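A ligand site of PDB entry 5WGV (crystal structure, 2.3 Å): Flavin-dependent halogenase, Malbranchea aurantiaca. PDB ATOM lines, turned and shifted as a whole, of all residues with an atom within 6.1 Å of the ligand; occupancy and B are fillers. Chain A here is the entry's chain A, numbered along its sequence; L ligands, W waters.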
ATOM      1  N   PRO A  85     -15.759  19.643 -21.312  1.00  0.00           N
ATOM      2  CA  PRO A  85     -15.334  19.623 -22.725  1.00  0.00           C
ATOM      3  C   PRO A  85     -15.441  20.967 -23.452  1.00  0.00           C
ATOM      4  O   PRO A  85     -14.612  21.230 -24.334  1.00  0.00           O
ATOM      5  CB  PRO A  85     -16.270  18.576 -23.338  1.00  0.00           C
ATOM      6  CG  PRO A  85     -16.501  17.602 -22.223  1.00  0.00           C
ATOM      7  CD  PRO A  85     -16.543  18.431 -20.965  1.00  0.00           C
ATOM      8  N   GLY A 110     -14.601  12.445 -17.257  1.00  0.00           N
ATOM      9  CA  GLY A 110     -15.993  12.293 -16.878  1.00  0.00           C
ATOM     10  C   GLY A 110     -16.297  12.564 -15.415  1.00  0.00           C
ATOM     11  O   GLY A 110     -15.473  13.078 -14.635  1.00  0.00           O
ATOM     12  N   LEU A 111     -17.529  12.208 -15.047  1.00  0.00           N
ATOM     13  CA  LEU A 111     -18.107  12.543 -13.753  1.00  0.00           C
ATOM     14  C   LEU A 111     -18.697  11.289 -13.130  1.00  0.00           C
ATOM     15  O   LEU A 111     -19.231  10.415 -13.834  1.00  0.00           O
ATOM     16  CB  LEU A 111     -19.197  13.621 -13.872  1.00  0.00           C
ATOM     17  CG  LEU A 111     -18.865  15.058 -14.283  1.00  0.00           C
ATOM     18  CD1 LEU A 111     -18.725  15.196 -15.785  1.00  0.00           C
ATOM     19  CD2 LEU A 111     -19.921  16.020 -13.759  1.00  0.00           C
ATOM     20  N   SER A 129     -20.140   8.095 -15.466  1.00  0.00           N
ATOM     21  CA  SER A 129     -19.987   8.362 -16.889  1.00  0.00           C
ATOM     22  C   SER A 129     -18.503   8.447 -17.219  1.00  0.00           C
ATOM     23  O   SER A 129     -17.650   8.478 -16.333  1.00  0.00           O
ATOM     24  CB  SER A 129     -20.713   9.639 -17.314  1.00  0.00           C
ATOM     25  OG  SER A 129     -19.952  10.796 -16.983  1.00  0.00           O
ATOM     26  N   VAL A 130     -18.194   8.492 -18.509  1.00  0.00           N
ATOM     27  CA  VAL A 130     -16.800   8.585 -18.961  1.00  0.00           C
ATOM     28  C   VAL A 130     -16.548   9.936 -19.604  1.00  0.00           C
ATOM     29  O   VAL A 130     -17.458  10.751 -19.749  1.00  0.00           O
ATOM     30  CB  VAL A 130     -16.448   7.450 -19.930  1.00  0.00           C
ATOM     31  CG1 VAL A 130     -16.536   6.112 -19.234  1.00  0.00           C
ATOM     32  CG2 VAL A 130     -17.365   7.484 -21.156  1.00  0.00           C
ATOM     33  N   GLY A 131     -15.291  10.179 -19.986  1.00  0.00           N
ATOM     34  CA  GLY A 131     -14.949  11.300 -20.836  1.00  0.00           C
ATOM     35  C   GLY A 131     -14.922  10.891 -22.298  1.00  0.00           C
ATOM     36  O   GLY A 131     -15.949  10.532 -22.874  1.00  0.00           O
ATOM     37  N   ALA A 132     -13.740  10.930 -22.911  1.00  0.00           N
ATOM     38  CA  ALA A 132     -13.600  10.692 -24.335  1.00  0.00           C
ATOM     39  C   ALA A 132     -12.264  10.007 -24.577  1.00  0.00           C
ATOM     40  O   ALA A 132     -11.386  10.040 -23.718  1.00  0.00           O
ATOM     41  CB  ALA A 132     -13.699  11.995 -25.133  1.00  0.00           C
ATOM     42  N   PRO A 133     -12.101   9.341 -25.728  1.00  0.00           N
ATOM     43  CA  PRO A 133     -10.772   8.825 -26.099  1.00  0.00           C
ATOM     44  C   PRO A 133      -9.742   9.946 -26.201  1.00  0.00           C
ATOM     45  O   PRO A 133     -10.067  11.097 -26.513  1.00  0.00           O
ATOM     46  CB  PRO A 133     -11.017   8.166 -27.464  1.00  0.00           C
ATOM     47  CG  PRO A 133     -12.450   7.818 -27.460  1.00  0.00           C
ATOM     48  CD  PRO A 133     -13.154   8.862 -26.640  1.00  0.00           C
ATOM     49  N   VAL A 136      -9.827  12.211 -29.094  1.00  0.00           N
ATOM     50  CA  VAL A 136     -11.047  12.978 -29.299  1.00  0.00           C
ATOM     51  C   VAL A 136     -10.913  14.308 -28.565  1.00  0.00           C
ATOM     52  O   VAL A 136     -10.695  15.353 -29.205  1.00  0.00           O
ATOM     53  CB  VAL A 136     -12.279  12.180 -28.821  1.00  0.00           C
ATOM     54  CG1 VAL A 136     -13.545  13.003 -28.984  1.00  0.00           C
ATOM     55  CG2 VAL A 136     -12.374  10.871 -29.594  1.00  0.00           C
ATOM     56  N   LEU A 137     -11.018  14.285 -27.243  1.00  0.00           N
ATOM     57  CA  LEU A 137     -10.803  15.475 -26.416  1.00  0.00           C
ATOM     58  C   LEU A 137     -10.426  15.025 -25.006  1.00  0.00           C
ATOM     59  O   LEU A 137     -10.268  13.827 -24.720  1.00  0.00           O
ATOM     60  CB  LEU A 137     -12.033  16.383 -26.418  1.00  0.00           C
ATOM     61  CG  LEU A 137     -13.415  15.873 -25.982  1.00  0.00           C
ATOM     62  CD1 LEU A 137     -13.536  15.801 -24.454  1.00  0.00           C
ATOM     63  CD2 LEU A 137     -14.531  16.743 -26.554  1.00  0.00           C
ATOM     64  N   PHE A 489     -27.529  14.785 -17.799  1.00  0.00           N
ATOM     65  CA  PHE A 489     -26.664  14.304 -18.868  1.00  0.00           C
ATOM     66  C   PHE A 489     -27.407  14.242 -20.207  1.00  0.00           C
ATOM     67  O   PHE A 489     -26.836  14.605 -21.246  1.00  0.00           O
ATOM     68  CB  PHE A 489     -26.092  12.947 -18.498  1.00  0.00           C
ATOM     69  CG  PHE A 489     -24.978  13.016 -17.487  1.00  0.00           C
ATOM     70  CD1 PHE A 489     -25.220  13.478 -16.200  1.00  0.00           C
ATOM     71  CD2 PHE A 489     -23.708  12.614 -17.815  1.00  0.00           C
ATOM     72  CE1 PHE A 489     -24.201  13.544 -15.279  1.00  0.00           C
ATOM     73  CE2 PHE A 489     -22.681  12.677 -16.897  1.00  0.00           C
ATOM     74  CZ  PHE A 489     -22.927  13.142 -15.629  1.00  0.00           C
ATOM     75  N   GLY A 492     -27.938  17.926 -21.203  1.00  0.00           N
ATOM     76  CA  GLY A 492     -26.776  18.796 -21.254  1.00  0.00           C
ATOM     77  C   GLY A 492     -25.545  18.271 -21.956  1.00  0.00           C
ATOM     78  O   GLY A 492     -24.505  18.939 -21.974  1.00  0.00           O
ATOM     79  N   ILE A 493     -25.617  17.080 -22.539  1.00  0.00           N
ATOM     80  CA  ILE A 493     -24.474  16.611 -23.304  1.00  0.00           C
ATOM     81  C   ILE A 493     -24.283  17.531 -24.521  1.00  0.00           C
ATOM     82  O   ILE A 493     -25.244  18.101 -25.056  1.00  0.00           O
ATOM     83  CB  ILE A 493     -24.658  15.129 -23.692  1.00  0.00           C
ATOM     84  CG1 ILE A 493     -23.367  14.565 -24.270  1.00  0.00           C
ATOM     85  CG2 ILE A 493     -25.858  14.946 -24.614  1.00  0.00           C
ATOM     86  CD1 ILE A 493     -23.157  13.111 -23.902  1.00  0.00           C
ATOM     87  N   GLU A 494     -23.021  17.730 -24.911  1.00  0.00           N
ATOM     88  CA  GLU A 494     -22.669  18.819 -25.831  1.00  0.00           C
ATOM     89  C   GLU A 494     -22.708  18.327 -27.278  1.00  0.00           C
ATOM     90  O   GLU A 494     -21.680  18.103 -27.932  1.00  0.00           O
ATOM     91  CB  GLU A 494     -21.290  19.376 -25.464  1.00  0.00           C
ATOM     92  CG  GLU A 494     -21.152  19.866 -24.013  1.00  0.00           C
ATOM     93  CD  GLU A 494     -20.513  18.832 -23.077  1.00  0.00           C
ATOM     94  OE1 GLU A 494     -20.752  17.611 -23.253  1.00  0.00           O
ATOM     95  OE2 GLU A 494     -19.767  19.248 -22.165  1.00  0.00           O
ATOM     96  N   ARG A 495     -23.925  18.157 -27.785  1.00  0.00           N
ATOM     97  CA  ARG A 495     -24.127  17.695 -29.152  1.00  0.00           C
ATOM     98  C   ARG A 495     -23.509  18.665 -30.151  1.00  0.00           C
ATOM     99  O   ARG A 495     -23.704  19.884 -30.058  1.00  0.00           O
ATOM    100  CB  ARG A 495     -25.627  17.525 -29.437  1.00  0.00           C
ATOM    101  CG  ARG A 495     -26.365  16.519 -28.537  1.00  0.00           C
ATOM    102  CD  ARG A 495     -27.893  16.656 -28.642  1.00  0.00           C
ATOM    103  NE  ARG A 495     -28.604  15.696 -27.805  1.00  0.00           N
ATOM    104  CZ  ARG A 495     -28.785  15.817 -26.493  1.00  0.00           C
ATOM    105  NH1 ARG A 495     -28.294  16.880 -25.843  1.00  0.00           N
ATOM    106  NH2 ARG A 495     -29.448  14.883 -25.811  1.00  0.00           N
ATOM    107  N   LEU A 497     -20.416  19.541 -30.569  1.00  0.00           N
ATOM    108  CA  LEU A 497     -19.309  20.367 -30.089  1.00  0.00           C
ATOM    109  C   LEU A 497     -18.129  20.343 -31.056  1.00  0.00           C
ATOM    110  O   LEU A 497     -17.369  21.324 -31.139  1.00  0.00           O
ATOM    111  CB  LEU A 497     -18.863  19.883 -28.702  1.00  0.00           C
ATOM    112  CG  LEU A 497     -17.699  20.557 -27.988  1.00  0.00           C
ATOM    113  CD1 LEU A 497     -17.943  22.054 -27.818  1.00  0.00           C
ATOM    114  CD2 LEU A 497     -17.460  19.903 -26.625  1.00  0.00           C
ATOM    115  N   TRP A 514     -25.919  23.839 -19.774  1.00  0.00           N
ATOM    116  CA  TRP A 514     -25.947  22.478 -19.212  1.00  0.00           C
ATOM    117  C   TRP A 514     -27.285  21.781 -19.444  1.00  0.00           C
ATOM    118  O   TRP A 514     -27.630  20.839 -18.723  1.00  0.00           O
ATOM    119  CB  TRP A 514     -25.630  22.487 -17.705  1.00  0.00           C
ATOM    120  CG  TRP A 514     -24.321  21.827 -17.330  1.00  0.00           C
ATOM    121  CD1 TRP A 514     -23.231  22.420 -16.765  1.00  0.00           C
ATOM    122  CD2 TRP A 514     -23.974  20.432 -17.491  1.00  0.00           C
ATOM    123  NE1 TRP A 514     -22.230  21.496 -16.568  1.00  0.00           N
ATOM    124  CE2 TRP A 514     -22.663  20.274 -17.007  1.00  0.00           C
ATOM    125  CE3 TRP A 514     -24.648  19.319 -18.006  1.00  0.00           C
ATOM    126  CZ2 TRP A 514     -21.998  19.034 -17.020  1.00  0.00           C
ATOM    127  CZ3 TRP A 514     -23.997  18.095 -18.012  1.00  0.00           C
ATOM    128  CH2 TRP A 514     -22.685  17.968 -17.524  1.00  0.00           C
ATOM    129  N   LEU A 568     -25.789   8.487 -30.431  1.00  0.00           N
ATOM    130  CA  LEU A 568     -24.927   8.464 -29.252  1.00  0.00           C
ATOM    131  C   LEU A 568     -24.952   7.058 -28.667  1.00  0.00           C
ATOM    132  O   LEU A 568     -26.021   6.541 -28.346  1.00  0.00           O
ATOM    133  CB  LEU A 568     -25.411   9.483 -28.234  1.00  0.00           C
ATOM    134  CG  LEU A 568     -24.427  10.434 -27.544  1.00  0.00           C
ATOM    135  CD1 LEU A 568     -23.153  10.644 -28.354  1.00  0.00           C
ATOM    136  CD2 LEU A 568     -25.132  11.749 -27.320  1.00  0.00           C
ATOM    137  N   ILE A 573     -21.435   5.246 -22.571  1.00  0.00           N
ATOM    138  CA  ILE A 573     -21.101   6.476 -21.863  1.00  0.00           C
ATOM    139  C   ILE A 573     -21.586   6.440 -20.410  1.00  0.00           C
ATOM    140  O   ILE A 573     -20.884   6.904 -19.511  1.00  0.00           O
ATOM    141  CB  ILE A 573     -21.685   7.691 -22.608  1.00  0.00           C
ATOM    142  CG1 ILE A 573     -21.124   7.762 -24.034  1.00  0.00           C
ATOM    143  CG2 ILE A 573     -21.390   8.975 -21.872  1.00  0.00           C
ATOM    144  CD1 ILE A 573     -21.790   8.832 -24.884  1.00  0.00           C
ATOM    145  N   LEU A 574     -22.787   5.912 -20.181  1.00  0.00           N
ATOM    146  CA  LEU A 574     -23.349   5.782 -18.838  1.00  0.00           C
ATOM    147  C   LEU A 574     -23.278   4.311 -18.435  1.00  0.00           C
ATOM    148  O   LEU A 574     -23.848   3.449 -19.127  1.00  0.00           O
ATOM    149  CB  LEU A 574     -24.781   6.301 -18.794  1.00  0.00           C
ATOM    150  CG  LEU A 574     -24.947   7.709 -19.359  1.00  0.00           C
ATOM    151  CD1 LEU A 574     -26.362   8.229 -19.090  1.00  0.00           C
ATOM    152  CD2 LEU A 574     -23.894   8.685 -18.789  1.00  0.00           C
ATOM    153  N   TYR A 593     -11.150   4.722 -21.367  1.00  0.00           N
ATOM    154  CA  TYR A 593     -10.310   5.681 -22.072  1.00  0.00           C
ATOM    155  C   TYR A 593      -9.018   6.003 -21.352  1.00  0.00           C
ATOM    156  O   TYR A 593      -8.132   6.632 -21.951  1.00  0.00           O
ATOM    157  CB  TYR A 593     -11.080   6.992 -22.292  1.00  0.00           C
ATOM    158  CG  TYR A 593     -12.376   6.845 -23.067  1.00  0.00           C
ATOM    159  CD1 TYR A 593     -12.488   5.951 -24.117  1.00  0.00           C
ATOM    160  CD2 TYR A 593     -13.487   7.615 -22.725  1.00  0.00           C
ATOM    161  CE1 TYR A 593     -13.677   5.826 -24.824  1.00  0.00           C
ATOM    162  CE2 TYR A 593     -14.673   7.500 -23.431  1.00  0.00           C
ATOM    163  CZ  TYR A 593     -14.773   6.601 -24.474  1.00  0.00           C
ATOM    164  OH  TYR A 593     -15.951   6.492 -25.160  1.00  0.00           O
ATOM    165  N   LEU A 641     -14.476   8.183 -35.946  1.00  0.00           N
ATOM    166  CA  LEU A 641     -14.637   8.927 -34.700  1.00  0.00           C
ATOM    167  C   LEU A 641     -13.525   9.961 -34.523  1.00  0.00           C
ATOM    168  O   LEU A 641     -13.788  11.160 -34.415  1.00  0.00           O
ATOM    169  CB  LEU A 641     -14.666   7.963 -33.512  1.00  0.00           C
ATOM    170  CG  LEU A 641     -14.578   8.579 -32.111  1.00  0.00           C
ATOM    171  CD1 LEU A 641     -15.715   9.566 -31.865  1.00  0.00           C
ATOM    172  CD2 LEU A 641     -14.579   7.485 -31.045  1.00  0.00           C
ATOM    173  N   TRP A 645     -12.821  14.801 -34.771  1.00  0.00           N
ATOM    174  CA  TRP A 645     -12.317  15.597 -33.663  1.00  0.00           C
ATOM    175  C   TRP A 645     -10.889  16.087 -33.864  1.00  0.00           C
ATOM    176  O   TRP A 645     -10.301  16.674 -32.936  1.00  0.00           O
ATOM    177  CB  TRP A 645     -12.415  14.789 -32.370  1.00  0.00           C
ATOM    178  CG  TRP A 645     -13.833  14.622 -31.954  1.00  0.00           C
ATOM    179  CD1 TRP A 645     -14.659  13.582 -32.260  1.00  0.00           C
ATOM    180  CD2 TRP A 645     -14.605  15.545 -31.187  1.00  0.00           C
ATOM    181  NE1 TRP A 645     -15.896  13.800 -31.708  1.00  0.00           N
ATOM    182  CE2 TRP A 645     -15.891  14.998 -31.033  1.00  0.00           C
ATOM    183  CE3 TRP A 645     -14.324  16.790 -30.589  1.00  0.00           C
ATOM    184  CZ2 TRP A 645     -16.908  15.639 -30.328  1.00  0.00           C
ATOM    185  CZ3 TRP A 645     -15.322  17.424 -29.890  1.00  0.00           C
ATOM    186  CH2 TRP A 645     -16.602  16.856 -29.762  1.00  0.00           C
HETATM  187  N1  LIG L   1     -17.165  11.042 -25.673  1.00  0.00           N
HETATM  188  C1  LIG L   1     -16.754  11.082 -26.949  1.00  0.00           C
HETATM  189  O1  LIG L   1     -15.823  10.412 -27.374  1.00  0.00           O
HETATM  190  C2  LIG L   1     -17.568  12.065 -27.794  1.00  0.00           C
HETATM  191  C3  LIG L   1     -21.571  14.098 -19.935  1.00  0.00           C
HETATM  192  C4  LIG L   1     -21.257  14.974 -20.962  1.00  0.00           C
HETATM  193  C5  LIG L   1     -20.497  14.497 -22.023  1.00  0.00           C
HETATM  194  C6  LIG L   1     -19.308  14.239 -23.897  1.00  0.00           C
HETATM  195  C7  LIG L   1     -18.644  14.586 -25.214  1.00  0.00           C
HETATM  196  C8  LIG L   1     -19.754  14.970 -26.198  1.00  0.00           C
HETATM  197  C9  LIG L   1     -17.767  15.825 -24.985  1.00  0.00           C
HETATM  198  C10 LIG L   1     -19.429  11.507 -26.253  1.00  0.00           C
HETATM  199  C11 LIG L   1     -19.067  10.511 -28.512  1.00  0.00           C
HETATM  200  C12 LIG L   1     -18.372  10.950 -29.792  1.00  0.00           C
HETATM  201  C13 LIG L   1     -17.373  13.455 -27.171  1.00  0.00           C
HETATM  202  C14 LIG L   1     -17.308  11.939 -29.306  1.00  0.00           C
HETATM  203  C15 LIG L   1     -17.786  13.371 -25.682  1.00  0.00           C
HETATM  204  C16 LIG L   1     -18.291  11.923 -25.321  1.00  0.00           C
HETATM  205  C17 LIG L   1     -18.582  11.826 -23.814  1.00  0.00           C
HETATM  206  C18 LIG L   1     -19.295  13.019 -23.283  1.00  0.00           C
HETATM  207  C19 LIG L   1     -20.063  13.160 -22.072  1.00  0.00           C
HETATM  208  C20 LIG L   1     -20.401  12.303 -21.036  1.00  0.00           C
HETATM  209  C21 LIG L   1     -21.152  12.776 -19.978  1.00  0.00           C
HETATM  210  N2  LIG L   1     -20.025  15.144 -23.148  1.00  0.00           N
HETATM  211  N3  LIG L   1     -18.987  11.682 -27.642  1.00  0.00           N
HETATM  212  O   HOH W   1     -16.686  13.961 -22.003  1.00  0.00           O
HETATM  213  O   HOH W   2     -18.626  12.771 -32.446  1.00  0.00           O
HETATM  214  O   HOH W   3     -19.309   7.317 -29.212  1.00  0.00           O
HETATM  215  O   HOH W   4     -19.650  17.309 -19.921  1.00  0.00           O
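N2 of the ligand is in hydrogen-bond range of OE1 of Glu 494, 2.6 Å away. The backbone carbonyl oxygen (O) of Gly 131 sits close to a nitrogen (N1) of the ligand, 3.1 Å away.
The backbone carbonyl oxygen (O) of Ile 493 lies close to the guanidinium group (NH1) of Arg 495, at 3.4 Å. The backbone NH (N) of Val 130 is in hydrogen-bond range of the backbone carbonyl oxygen (O) of Ile 573, at 3.3 Å. The backbone NH (N) of Ser 129 lies within hydrogen-bond range of the backbone carbonyl oxygen (O) of Leu 111 (3.0 Å).
CG of Pro 85 touches C9 of the ligand, at 3.5 Å. Ser 129 touches the ligand (OG to C21, 3.8 Å). O of Val 130 touches C20 of the ligand, 3.6 Å away. CB of Ala 132 touches O1 of the ligand (3.5 Å). Pro 133 touches the ligand. CG1 of Val 136 touches O1 of the ligand (3.8 Å). Leu 137 touches the ligand (CD2 to C9, 3.7 Å). Phe 489 touches the ligand (CD2 to C21, 3.4 Å). Ile 493 touches the ligand. Ile 573 touches the ligand (CG2 to C20, 3.6 Å). CD1 of Leu 641 touches C12 of the ligand (3.6 Å). Trp 645 touches the ligand. Within 4 Å of the ligand: Pro 85, Ser 129, Val 130, Gly 131, Ala 132, Pro 133, Val 136, Leu 137, Phe 489, Ile 493, Glu 494, Ile 573, Leu 641 and Trp 645. The nearest printed residue that does not touch the ligand is Leu 568 (4.1 Å).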
